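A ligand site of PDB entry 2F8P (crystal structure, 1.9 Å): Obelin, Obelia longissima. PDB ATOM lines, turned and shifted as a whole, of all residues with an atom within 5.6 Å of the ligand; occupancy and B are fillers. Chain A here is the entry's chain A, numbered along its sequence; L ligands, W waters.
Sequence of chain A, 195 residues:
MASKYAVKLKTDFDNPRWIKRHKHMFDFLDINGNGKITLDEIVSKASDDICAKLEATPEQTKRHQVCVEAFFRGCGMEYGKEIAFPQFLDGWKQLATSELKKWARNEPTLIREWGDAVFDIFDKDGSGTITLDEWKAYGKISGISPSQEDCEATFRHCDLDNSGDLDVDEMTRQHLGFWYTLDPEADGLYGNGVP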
ATOM      1  N   ARG A  21     -21.110 -23.313  28.273  1.00  0.00           N
ATOM      2  CA  ARG A  21     -21.555 -22.182  27.434  1.00  0.00           C
ATOM      3  C   ARG A  21     -20.579 -21.017  27.510  1.00  0.00           C
ATOM      4  O   ARG A  21     -20.237 -20.414  26.491  1.00  0.00           O
ATOM      5  CB  ARG A  21     -22.972 -21.736  27.841  1.00  0.00           C
ATOM      6  CG  ARG A  21     -24.082 -22.645  27.289  1.00  0.00           C
ATOM      7  CD  ARG A  21     -25.429 -22.190  27.812  1.00  0.00           C
ATOM      8  NE  ARG A  21     -26.485 -23.107  27.389  1.00  0.00           N
ATOM      9  CZ  ARG A  21     -27.784 -22.884  27.522  1.00  0.00           C
ATOM     10  NH1 ARG A  21     -28.223 -21.749  28.063  1.00  0.00           N
ATOM     11  NH2 ARG A  21     -28.653 -23.800  27.110  1.00  0.00           N
ATOM     12  N   HIS A  22     -20.146 -20.681  28.707  1.00  0.00           N
ATOM     13  CA  HIS A  22     -19.207 -19.598  28.911  1.00  0.00           C
ATOM     14  C   HIS A  22     -17.803 -19.954  28.480  1.00  0.00           C
ATOM     15  O   HIS A  22     -17.079 -19.087  27.978  1.00  0.00           O
ATOM     16  CB  HIS A  22     -19.272 -19.126  30.352  1.00  0.00           C
ATOM     17  CG  HIS A  22     -20.526 -18.356  30.618  1.00  0.00           C
ATOM     18  ND1 HIS A  22     -20.717 -17.099  30.095  1.00  0.00           N
ATOM     19  CD2 HIS A  22     -21.657 -18.659  31.283  1.00  0.00           C
ATOM     20  CE1 HIS A  22     -21.911 -16.653  30.458  1.00  0.00           C
ATOM     21  NE2 HIS A  22     -22.514 -17.587  31.161  1.00  0.00           N
ATOM     22  N   MET A  25     -17.570 -19.472  24.766  1.00  0.00           N
ATOM     23  CA  MET A  25     -17.414 -18.028  24.468  1.00  0.00           C
ATOM     24  C   MET A  25     -16.033 -17.452  24.791  1.00  0.00           C
ATOM     25  O   MET A  25     -15.477 -16.712  23.994  1.00  0.00           O
ATOM     26  CB  MET A  25     -18.562 -17.194  25.086  1.00  0.00           C
ATOM     27  CG  MET A  25     -19.904 -17.577  24.490  1.00  0.00           C
ATOM     28  SD  MET A  25     -20.018 -17.300  22.712  1.00  0.00           S
ATOM     29  CE  MET A  25     -19.767 -15.517  22.601  1.00  0.00           C
ATOM     30  N   PHE A  26     -15.474 -17.832  25.940  1.00  0.00           N
ATOM     31  CA  PHE A  26     -14.136 -17.399  26.350  1.00  0.00           C
ATOM     32  C   PHE A  26     -13.107 -17.748  25.266  1.00  0.00           C
ATOM     33  O   PHE A  26     -12.347 -16.858  24.809  1.00  0.00           O
ATOM     34  CB  PHE A  26     -13.777 -18.037  27.718  1.00  0.00           C
ATOM     35  CG  PHE A  26     -12.417 -17.684  28.244  1.00  0.00           C
ATOM     36  CD1 PHE A  26     -12.247 -16.668  29.172  1.00  0.00           C
ATOM     37  CD2 PHE A  26     -11.283 -18.406  27.814  1.00  0.00           C
ATOM     38  CE1 PHE A  26     -10.972 -16.344  29.684  1.00  0.00           C
ATOM     39  CE2 PHE A  26     -10.021 -18.081  28.282  1.00  0.00           C
ATOM     40  CZ  PHE A  26      -9.852 -17.048  29.229  1.00  0.00           C
ATOM     41  N   PHE A  28     -13.750 -18.589  22.067  1.00  0.00           N
ATOM     42  CA  PHE A  28     -14.106 -17.842  20.862  1.00  0.00           C
ATOM     43  C   PHE A  28     -13.562 -16.405  20.905  1.00  0.00           C
ATOM     44  O   PHE A  28     -13.027 -15.907  19.890  1.00  0.00           O
ATOM     45  CB  PHE A  28     -15.645 -17.791  20.711  1.00  0.00           C
ATOM     46  CG  PHE A  28     -16.109 -16.948  19.543  1.00  0.00           C
ATOM     47  CD1 PHE A  28     -15.919 -17.381  18.219  1.00  0.00           C
ATOM     48  CD2 PHE A  28     -16.744 -15.718  19.764  1.00  0.00           C
ATOM     49  CE1 PHE A  28     -16.356 -16.594  17.146  1.00  0.00           C
ATOM     50  CE2 PHE A  28     -17.181 -14.935  18.699  1.00  0.00           C
ATOM     51  CZ  PHE A  28     -17.000 -15.377  17.383  1.00  0.00           C
ATOM     52  N   LEU A  29     -13.731 -15.733  22.044  1.00  0.00           N
ATOM     53  CA  LEU A  29     -13.330 -14.338  22.211  1.00  0.00           C
ATOM     54  C   LEU A  29     -11.812 -14.118  22.449  1.00  0.00           C
ATOM     55  O   LEU A  29     -11.310 -12.987  22.299  1.00  0.00           O
ATOM     56  CB  LEU A  29     -14.120 -13.674  23.336  1.00  0.00           C
ATOM     57  CG  LEU A  29     -15.658 -13.668  23.174  1.00  0.00           C
ATOM     58  CD1 LEU A  29     -16.317 -13.244  24.459  1.00  0.00           C
ATOM     59  CD2 LEU A  29     -16.073 -12.781  22.049  1.00  0.00           C
ATOM     60  N   LYS A  45     -14.430  -8.543  19.338  1.00  0.00           N
ATOM     61  CA  LYS A  45     -15.270  -9.622  18.781  1.00  0.00           C
ATOM     62  C   LYS A  45     -16.775  -9.449  19.033  1.00  0.00           C
ATOM     63  O   LYS A  45     -17.590  -9.601  18.115  1.00  0.00           O
ATOM     64  CB  LYS A  45     -14.819 -10.988  19.316  1.00  0.00           C
ATOM     65  CG  LYS A  45     -13.481 -11.432  18.709  1.00  0.00           C
ATOM     66  CD  LYS A  45     -13.340 -12.961  18.655  1.00  0.00           C
ATOM     67  CE  LYS A  45     -13.606 -13.531  17.288  1.00  0.00           C
ATOM     68  NZ  LYS A  45     -13.184 -14.971  17.198  1.00  0.00           N
ATOM     69  N   ALA A  46     -17.142  -9.124  20.271  1.00  0.00           N
ATOM     70  CA  ALA A  46     -18.553  -9.024  20.654  1.00  0.00           C
ATOM     71  C   ALA A  46     -19.201  -7.662  20.306  1.00  0.00           C
ATOM     72  O   ALA A  46     -20.419  -7.536  20.324  1.00  0.00           O
ATOM     73  CB  ALA A  46     -18.719  -9.331  22.140  1.00  0.00           C
ATOM     74  N   ILE A  50     -19.396  -7.524  15.491  1.00  0.00           N
ATOM     75  CA  ILE A  50     -20.872  -7.615  15.449  1.00  0.00           C
ATOM     76  C   ILE A  50     -21.501  -6.342  14.846  1.00  0.00           C
ATOM     77  O   ILE A  50     -22.303  -6.420  13.919  1.00  0.00           O
ATOM     78  CB  ILE A  50     -21.490  -7.922  16.846  1.00  0.00           C
ATOM     79  CG1 ILE A  50     -21.105  -9.315  17.335  1.00  0.00           C
ATOM     80  CG2 ILE A  50     -23.064  -7.878  16.769  1.00  0.00           C
ATOM     81  CD1 ILE A  50     -21.846 -10.465  16.576  1.00  0.00           C
ATOM     82  N   PHE A  72     -19.331  -6.110  30.626  1.00  0.00           N
ATOM     83  CA  PHE A  72     -18.132  -6.895  30.943  1.00  0.00           C
ATOM     84  C   PHE A  72     -17.280  -6.357  32.060  1.00  0.00           C
ATOM     85  O   PHE A  72     -16.641  -7.142  32.723  1.00  0.00           O
ATOM     86  CB  PHE A  72     -17.348  -7.277  29.666  1.00  0.00           C
ATOM     87  CG  PHE A  72     -18.076  -8.330  28.854  1.00  0.00           C
ATOM     88  CD1 PHE A  72     -17.978  -9.677  29.222  1.00  0.00           C
ATOM     89  CD2 PHE A  72     -18.917  -7.976  27.815  1.00  0.00           C
ATOM     90  CE1 PHE A  72     -18.689 -10.673  28.516  1.00  0.00           C
ATOM     91  CE2 PHE A  72     -19.646  -8.946  27.088  1.00  0.00           C
ATOM     92  CZ  PHE A  72     -19.544 -10.301  27.452  1.00  0.00           C
ATOM     93  N   PHE A  88     -12.840 -15.250  35.079  1.00  0.00           N
ATOM     94  CA  PHE A  88     -13.851 -14.830  34.116  1.00  0.00           C
ATOM     95  C   PHE A  88     -15.208 -15.360  34.549  1.00  0.00           C
ATOM     96  O   PHE A  88     -16.197 -14.608  34.572  1.00  0.00           O
ATOM     97  CB  PHE A  88     -13.478 -15.300  32.697  1.00  0.00           C
ATOM     98  CG  PHE A  88     -14.471 -14.924  31.591  1.00  0.00           C
ATOM     99  CD1 PHE A  88     -14.474 -13.635  31.017  1.00  0.00           C
ATOM    100  CD2 PHE A  88     -15.334 -15.894  31.065  1.00  0.00           C
ATOM    101  CE1 PHE A  88     -15.355 -13.309  29.965  1.00  0.00           C
ATOM    102  CE2 PHE A  88     -16.220 -15.580  30.006  1.00  0.00           C
ATOM    103  CZ  PHE A  88     -16.228 -14.296  29.463  1.00  0.00           C
ATOM    104  N   TRP A  92     -18.762 -13.589  35.927  1.00  0.00           N
ATOM    105  CA  TRP A  92     -20.123 -13.852  35.422  1.00  0.00           C
ATOM    106  C   TRP A  92     -21.097 -14.255  36.551  1.00  0.00           C
ATOM    107  O   TRP A  92     -22.290 -13.880  36.546  1.00  0.00           O
ATOM    108  CB  TRP A  92     -20.090 -14.953  34.364  1.00  0.00           C
ATOM    109  CG  TRP A  92     -19.965 -14.474  32.962  1.00  0.00           C
ATOM    110  CD1 TRP A  92     -18.819 -14.384  32.215  1.00  0.00           C
ATOM    111  CD2 TRP A  92     -21.048 -14.045  32.104  1.00  0.00           C
ATOM    112  NE1 TRP A  92     -19.114 -13.888  30.955  1.00  0.00           N
ATOM    113  CE2 TRP A  92     -20.480 -13.683  30.868  1.00  0.00           C
ATOM    114  CE3 TRP A  92     -22.445 -13.922  32.277  1.00  0.00           C
ATOM    115  CZ2 TRP A  92     -21.259 -13.245  29.781  1.00  0.00           C
ATOM    116  CZ3 TRP A  92     -23.215 -13.493  31.219  1.00  0.00           C
ATOM    117  CH2 TRP A  92     -22.610 -13.154  29.971  1.00  0.00           C
ATOM    118  N   ILE A 111     -27.888  -6.086  31.103  1.00  0.00           N
ATOM    119  CA  ILE A 111     -28.223  -7.005  30.011  1.00  0.00           C
ATOM    120  C   ILE A 111     -29.370  -6.478  29.135  1.00  0.00           C
ATOM    121  O   ILE A 111     -29.366  -6.631  27.915  1.00  0.00           O
ATOM    122  CB  ILE A 111     -28.468  -8.486  30.537  1.00  0.00           C
ATOM    123  CG1 ILE A 111     -28.418  -9.506  29.384  1.00  0.00           C
ATOM    124  CG2 ILE A 111     -29.780  -8.620  31.362  1.00  0.00           C
ATOM    125  CD1 ILE A 111     -28.078 -10.953  29.880  1.00  0.00           C
ATOM    126  N   TRP A 114     -27.966  -3.743  26.872  1.00  0.00           N
ATOM    127  CA  TRP A 114     -27.284  -4.368  25.744  1.00  0.00           C
ATOM    128  C   TRP A 114     -28.306  -4.860  24.694  1.00  0.00           C
ATOM    129  O   TRP A 114     -28.190  -4.543  23.513  1.00  0.00           O
ATOM    130  CB  TRP A 114     -26.369  -5.485  26.256  1.00  0.00           C
ATOM    131  CG  TRP A 114     -25.458  -6.159  25.215  1.00  0.00           C
ATOM    132  CD1 TRP A 114     -25.239  -5.789  23.916  1.00  0.00           C
ATOM    133  CD2 TRP A 114     -24.646  -7.293  25.463  1.00  0.00           C
ATOM    134  NE1 TRP A 114     -24.354  -6.694  23.319  1.00  0.00           N
ATOM    135  CE2 TRP A 114     -23.965  -7.604  24.254  1.00  0.00           C
ATOM    136  CE3 TRP A 114     -24.428  -8.096  26.596  1.00  0.00           C
ATOM    137  CZ2 TRP A 114     -23.072  -8.668  24.147  1.00  0.00           C
ATOM    138  CZ3 TRP A 114     -23.539  -9.196  26.482  1.00  0.00           C
ATOM    139  CH2 TRP A 114     -22.881  -9.454  25.265  1.00  0.00           C
ATOM    140  N   GLY A 115     -29.317  -5.609  25.131  1.00  0.00           N
ATOM    141  CA  GLY A 115     -30.412  -6.018  24.288  1.00  0.00           C
ATOM    142  C   GLY A 115     -31.072  -4.862  23.506  1.00  0.00           C
ATOM    143  O   GLY A 115     -31.363  -5.026  22.325  1.00  0.00           O
ATOM    144  N   VAL A 118     -28.662  -3.855  20.579  1.00  0.00           N
ATOM    145  CA  VAL A 118     -28.723  -4.842  19.509  1.00  0.00           C
ATOM    146  C   VAL A 118     -30.073  -4.771  18.767  1.00  0.00           C
ATOM    147  O   VAL A 118     -30.137  -4.773  17.543  1.00  0.00           O
ATOM    148  CB  VAL A 118     -28.424  -6.275  20.057  1.00  0.00           C
ATOM    149  CG1 VAL A 118     -28.717  -7.355  19.010  1.00  0.00           C
ATOM    150  CG2 VAL A 118     -26.935  -6.402  20.539  1.00  0.00           C
ATOM    151  N   SER A 142     -23.833 -12.196  10.954  1.00  0.00           N
ATOM    152  CA  SER A 142     -23.294 -11.649  12.198  1.00  0.00           C
ATOM    153  C   SER A 142     -22.716 -12.731  13.094  1.00  0.00           C
ATOM    154  O   SER A 142     -21.965 -12.425  14.032  1.00  0.00           O
ATOM    155  CB  SER A 142     -24.397 -10.896  12.933  1.00  0.00           C
ATOM    156  OG  SER A 142     -25.326 -11.819  13.463  1.00  0.00           O
ATOM    157  N   GLY A 143     -23.073 -13.980  12.832  1.00  0.00           N
ATOM    158  CA  GLY A 143     -22.530 -15.111  13.582  1.00  0.00           C
ATOM    159  C   GLY A 143     -23.454 -15.647  14.657  1.00  0.00           C
ATOM    160  O   GLY A 143     -23.105 -16.602  15.359  1.00  0.00           O
ATOM    161  N   ILE A 144     -24.626 -15.039  14.787  1.00  0.00           N
ATOM    162  CA  ILE A 144     -25.641 -15.433  15.775  1.00  0.00           C
ATOM    163  C   ILE A 144     -26.346 -16.794  15.492  1.00  0.00           C
ATOM    164  O   ILE A 144     -26.611 -17.553  16.435  1.00  0.00           O
ATOM    165  CB  ILE A 144     -26.656 -14.286  16.057  1.00  0.00           C
ATOM    166  CG1 ILE A 144     -26.067 -13.260  17.045  1.00  0.00           C
ATOM    167  CG2 ILE A 144     -27.973 -14.805  16.640  1.00  0.00           C
ATOM    168  CD1 ILE A 144     -25.552 -11.962  16.441  1.00  0.00           C
ATOM    169  N   MET A 171     -36.716 -10.800  22.925  1.00  0.00           N
ATOM    170  CA  MET A 171     -35.305 -11.005  22.657  1.00  0.00           C
ATOM    171  C   MET A 171     -34.441 -10.978  23.914  1.00  0.00           C
ATOM    172  O   MET A 171     -33.656 -11.906  24.118  1.00  0.00           O
ATOM    173  CB  MET A 171     -34.787  -9.989  21.660  1.00  0.00           C
ATOM    174  CG  MET A 171     -33.335 -10.239  21.248  1.00  0.00           C
ATOM    175  SD  MET A 171     -32.879  -9.122  19.923  1.00  0.00           S
ATOM    176  CE  MET A 171     -32.337  -7.762  20.940  1.00  0.00           C
ATOM    177  N   THR A 172     -34.607  -9.936  24.733  1.00  0.00           N
ATOM    178  CA  THR A 172     -33.824  -9.766  25.961  1.00  0.00           C
ATOM    179  C   THR A 172     -34.037 -10.895  26.979  1.00  0.00           C
ATOM    180  O   THR A 172     -33.087 -11.379  27.643  1.00  0.00           O
ATOM    181  CB  THR A 172     -34.028  -8.314  26.612  1.00  0.00           C
ATOM    182  OG1 THR A 172     -35.417  -8.033  26.828  1.00  0.00           O
ATOM    183  CG2 THR A 172     -33.515  -7.242  25.676  1.00  0.00           C
ATOM    184  N   HIS A 175     -32.138 -13.932  25.711  1.00  0.00           N
ATOM    185  CA  HIS A 175     -30.709 -13.684  25.941  1.00  0.00           C
ATOM    186  C   HIS A 175     -30.363 -13.871  27.395  1.00  0.00           C
ATOM    187  O   HIS A 175     -29.370 -14.528  27.719  1.00  0.00           O
ATOM    188  CB  HIS A 175     -30.334 -12.245  25.473  1.00  0.00           C
ATOM    189  CG  HIS A 175     -28.860 -12.008  25.320  1.00  0.00           C
ATOM    190  ND1 HIS A 175     -28.175 -11.122  26.117  1.00  0.00           N
ATOM    191  CD2 HIS A 175     -27.969 -12.487  24.418  1.00  0.00           C
ATOM    192  CE1 HIS A 175     -26.904 -11.097  25.750  1.00  0.00           C
ATOM    193  NE2 HIS A 175     -26.757 -11.887  24.698  1.00  0.00           N
ATOM    194  N   TRP A 179     -27.790 -16.982  29.059  1.00  0.00           N
ATOM    195  CA  TRP A 179     -26.475 -16.665  29.657  1.00  0.00           C
ATOM    196  C   TRP A 179     -26.435 -16.572  31.203  1.00  0.00           C
ATOM    197  O   TRP A 179     -25.423 -16.924  31.821  1.00  0.00           O
ATOM    198  CB  TRP A 179     -25.942 -15.359  29.057  1.00  0.00           C
ATOM    199  CG  TRP A 179     -25.727 -15.457  27.586  1.00  0.00           C
ATOM    200  CD1 TRP A 179     -26.343 -14.728  26.629  1.00  0.00           C
ATOM    201  CD2 TRP A 179     -24.834 -16.364  26.899  1.00  0.00           C
ATOM    202  NE1 TRP A 179     -25.863 -15.077  25.391  1.00  0.00           N
ATOM    203  CE2 TRP A 179     -24.949 -16.087  25.532  1.00  0.00           C
ATOM    204  CE3 TRP A 179     -23.924 -17.355  27.327  1.00  0.00           C
ATOM    205  CZ2 TRP A 179     -24.194 -16.789  24.545  1.00  0.00           C
ATOM    206  CZ3 TRP A 179     -23.174 -18.053  26.353  1.00  0.00           C
ATOM    207  CH2 TRP A 179     -23.316 -17.769  24.990  1.00  0.00           C
ATOM    208  N   TYR A 190     -29.390 -19.801  19.993  1.00  0.00           N
ATOM    209  CA  TYR A 190     -28.279 -19.771  19.072  1.00  0.00           C
ATOM    210  C   TYR A 190     -28.272 -21.058  18.212  1.00  0.00           C
ATOM    211  O   TYR A 190     -27.216 -21.471  17.699  1.00  0.00           O
ATOM    212  CB  TYR A 190     -26.971 -19.594  19.846  1.00  0.00           C
ATOM    213  CG  TYR A 190     -26.853 -18.245  20.570  1.00  0.00           C
ATOM    214  CD1 TYR A 190     -27.099 -18.152  21.939  1.00  0.00           C
ATOM    215  CD2 TYR A 190     -26.502 -17.084  19.877  1.00  0.00           C
ATOM    216  CE1 TYR A 190     -26.979 -16.927  22.612  1.00  0.00           C
ATOM    217  CE2 TYR A 190     -26.396 -15.846  20.535  1.00  0.00           C
ATOM    218  CZ  TYR A 190     -26.651 -15.782  21.901  1.00  0.00           C
ATOM    219  OH  TYR A 190     -26.531 -14.602  22.565  1.00  0.00           O
HETATM  220  O1  LIG L   1     -25.705 -12.633  21.097  1.00  0.00           O
HETATM  221  C1  LIG L   1     -25.392 -11.434  21.102  1.00  0.00           C
HETATM  222  C2  LIG L   1     -26.266 -10.354  20.483  1.00  0.00           C
HETATM  223  C3  LIG L   1     -27.455 -10.086  21.394  1.00  0.00           C
HETATM  224  C4  LIG L   1     -28.694 -10.614  21.038  1.00  0.00           C
HETATM  225  C5  LIG L   1     -29.793 -10.384  21.874  1.00  0.00           C
HETATM  226  C6  LIG L   1     -29.628  -9.591  23.027  1.00  0.00           C
HETATM  227  O2  LIG L   1     -30.691  -9.376  23.834  1.00  0.00           O
HETATM  228  C7  LIG L   1     -28.380  -9.049  23.367  1.00  0.00           C
HETATM  229  C8  LIG L   1     -27.285  -9.301  22.543  1.00  0.00           C
HETATM  230  N1  LIG L   1     -24.225 -11.001  21.623  1.00  0.00           N
HETATM  231  C9  LIG L   1     -23.489 -11.679  22.538  1.00  0.00           C
HETATM  232  C10 LIG L   1     -22.118 -11.887  22.357  1.00  0.00           C
HETATM  233  C11 LIG L   1     -21.403 -11.416  21.095  1.00  0.00           C
HETATM  234  C12 LIG L   1     -21.477 -12.526  20.032  1.00  0.00           C
HETATM  235  C13 LIG L   1     -20.432 -12.697  19.114  1.00  0.00           C
HETATM  236  C14 LIG L   1     -20.503 -13.721  18.160  1.00  0.00           C
HETATM  237  C15 LIG L   1     -21.605 -14.580  18.077  1.00  0.00           C
HETATM  238  C16 LIG L   1     -22.642 -14.429  18.996  1.00  0.00           C
HETATM  239  C17 LIG L   1     -22.562 -13.397  19.943  1.00  0.00           C
HETATM  240  N2  LIG L   1     -21.427 -12.554  23.299  1.00  0.00           N
HETATM  241  C18 LIG L   1     -22.017 -13.016  24.432  1.00  0.00           C
HETATM  242  C19 LIG L   1     -23.374 -12.807  24.602  1.00  0.00           C
HETATM  243  N3  LIG L   1     -24.083 -12.144  23.647  1.00  0.00           N
HETATM  244  C20 LIG L   1     -21.209 -13.682  25.508  1.00  0.00           C
HETATM  245  C21 LIG L   1     -21.826 -14.656  26.303  1.00  0.00           C
HETATM  246  C22 LIG L   1     -21.099 -15.328  27.298  1.00  0.00           C
HETATM  247  C23 LIG L   1     -19.746 -15.009  27.474  1.00  0.00           C
HETATM  248  O3  LIG L   1     -19.060 -15.648  28.431  1.00  0.00           O
HETATM  249  C24 LIG L   1     -19.121 -14.016  26.700  1.00  0.00           C
HETATM  250  C25 LIG L   1     -19.857 -13.383  25.674  1.00  0.00           C
HETATM  251  O   HOH W   1     -29.954  -8.840  26.384  1.00  0.00           O
HETATM  252  O   HOH W   2     -23.227  -8.263  20.674  1.00  0.00           O
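Met 25 touches the ligand (CB to C23, 3.4 Å).
Phe 28 touches the ligand.
CD1 of Leu 29 touches C24 of the ligand, 3.7 Å away.
Ala 46 touches the ligand.
Ile 50 touches the ligand (CD1 to C13, 3.7 Å).
Phe 72 touches the ligand (CZ to C25, 3.6 Å).
Phe 88 touches the ligand (CE2 to O3, 3.2 Å).
Trp 114 touches the ligand.
CA of Gly 115 touches O2 of the ligand (3.4 Å).
Val 118 touches the ligand.
Gly 143 touches the ligand (O to C15, 3.7 Å).
Met 171 touches the ligand.
CA of Thr 172 touches O2 of the ligand, at 3.8 Å.
Trp 179 touches the ligand.
Hydrophobic or aromatic side chains within 4 Å of the ligand: His 22, Met 25, Phe 28, Leu 29, Ala 46, Ile 50, Phe 72, Phe 88, Trp 92, Trp 114, Val 118, Met 171, His 175, Trp 179 and Tyr 190.
18 residues have an atom within 4 Å of the ligand: His 22, Met 25, Phe 28, Leu 29, Ala 46, Ile 50, Phe 72, Phe 88, Trp 92, Trp 114, Gly 115, Val 118, Gly 143, Met 171, Thr 172, His 175, Trp 179 and Tyr 190.
Along chain A the residues within 4 Å of the ligand span positions 22 to 190.
The nearest printed residue that does not touch the ligand is Ile 144 (4.1 Å).
An oxygen (O3) of the ligand sits at hydrogen-bond distance from a ring nitrogen (ND1) of His 22.
NE1 of Trp 92 lies within hydrogen-bond range of O3 of the ligand (3.1 Å).
A ring nitrogen (NE2) of His 175 sits at hydrogen-bond distance from a nitrogen (N3) of the ligand, at 2.9 Å.
The side-chain hydroxyl (OH) of Tyr 190 is in hydrogen-bond range of an oxygen (O1) of the ligand (2.6 Å).
Water W1 lies within hydrogen-bond range of an oxygen (O2) of the ligand (2.7 Å), the backbone carbonyl oxygen of Ile 111 (2.8 Å) and a ring nitrogen (ND1) of His 175 (2.9 Å).
Water W2 lies within hydrogen-bond range of O of Ala 46 (2.9 Å), N1 of the ligand (3.1 Å) and NE1 of Trp 114 (3.3 Å).
A ring nitrogen (NE2) of His 175 sits at hydrogen-bond distance from the indole nitrogen (NE1) of Trp 179, at 3.4 Å.
The backbone carbonyl oxygen of Phe 28 is in hydrogen-bond range of the side-chain amino group of Lys 45.
NE2 of His 22 is in hydrogen-bond range of O of Trp 179, at 3.1 Å.
NE1 of Trp 179 is in hydrogen-bond range of OH of Tyr 190, 2.9 Å away.
NE2 of His 175 lies close to OH of Tyr 190 (3.5 Å).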
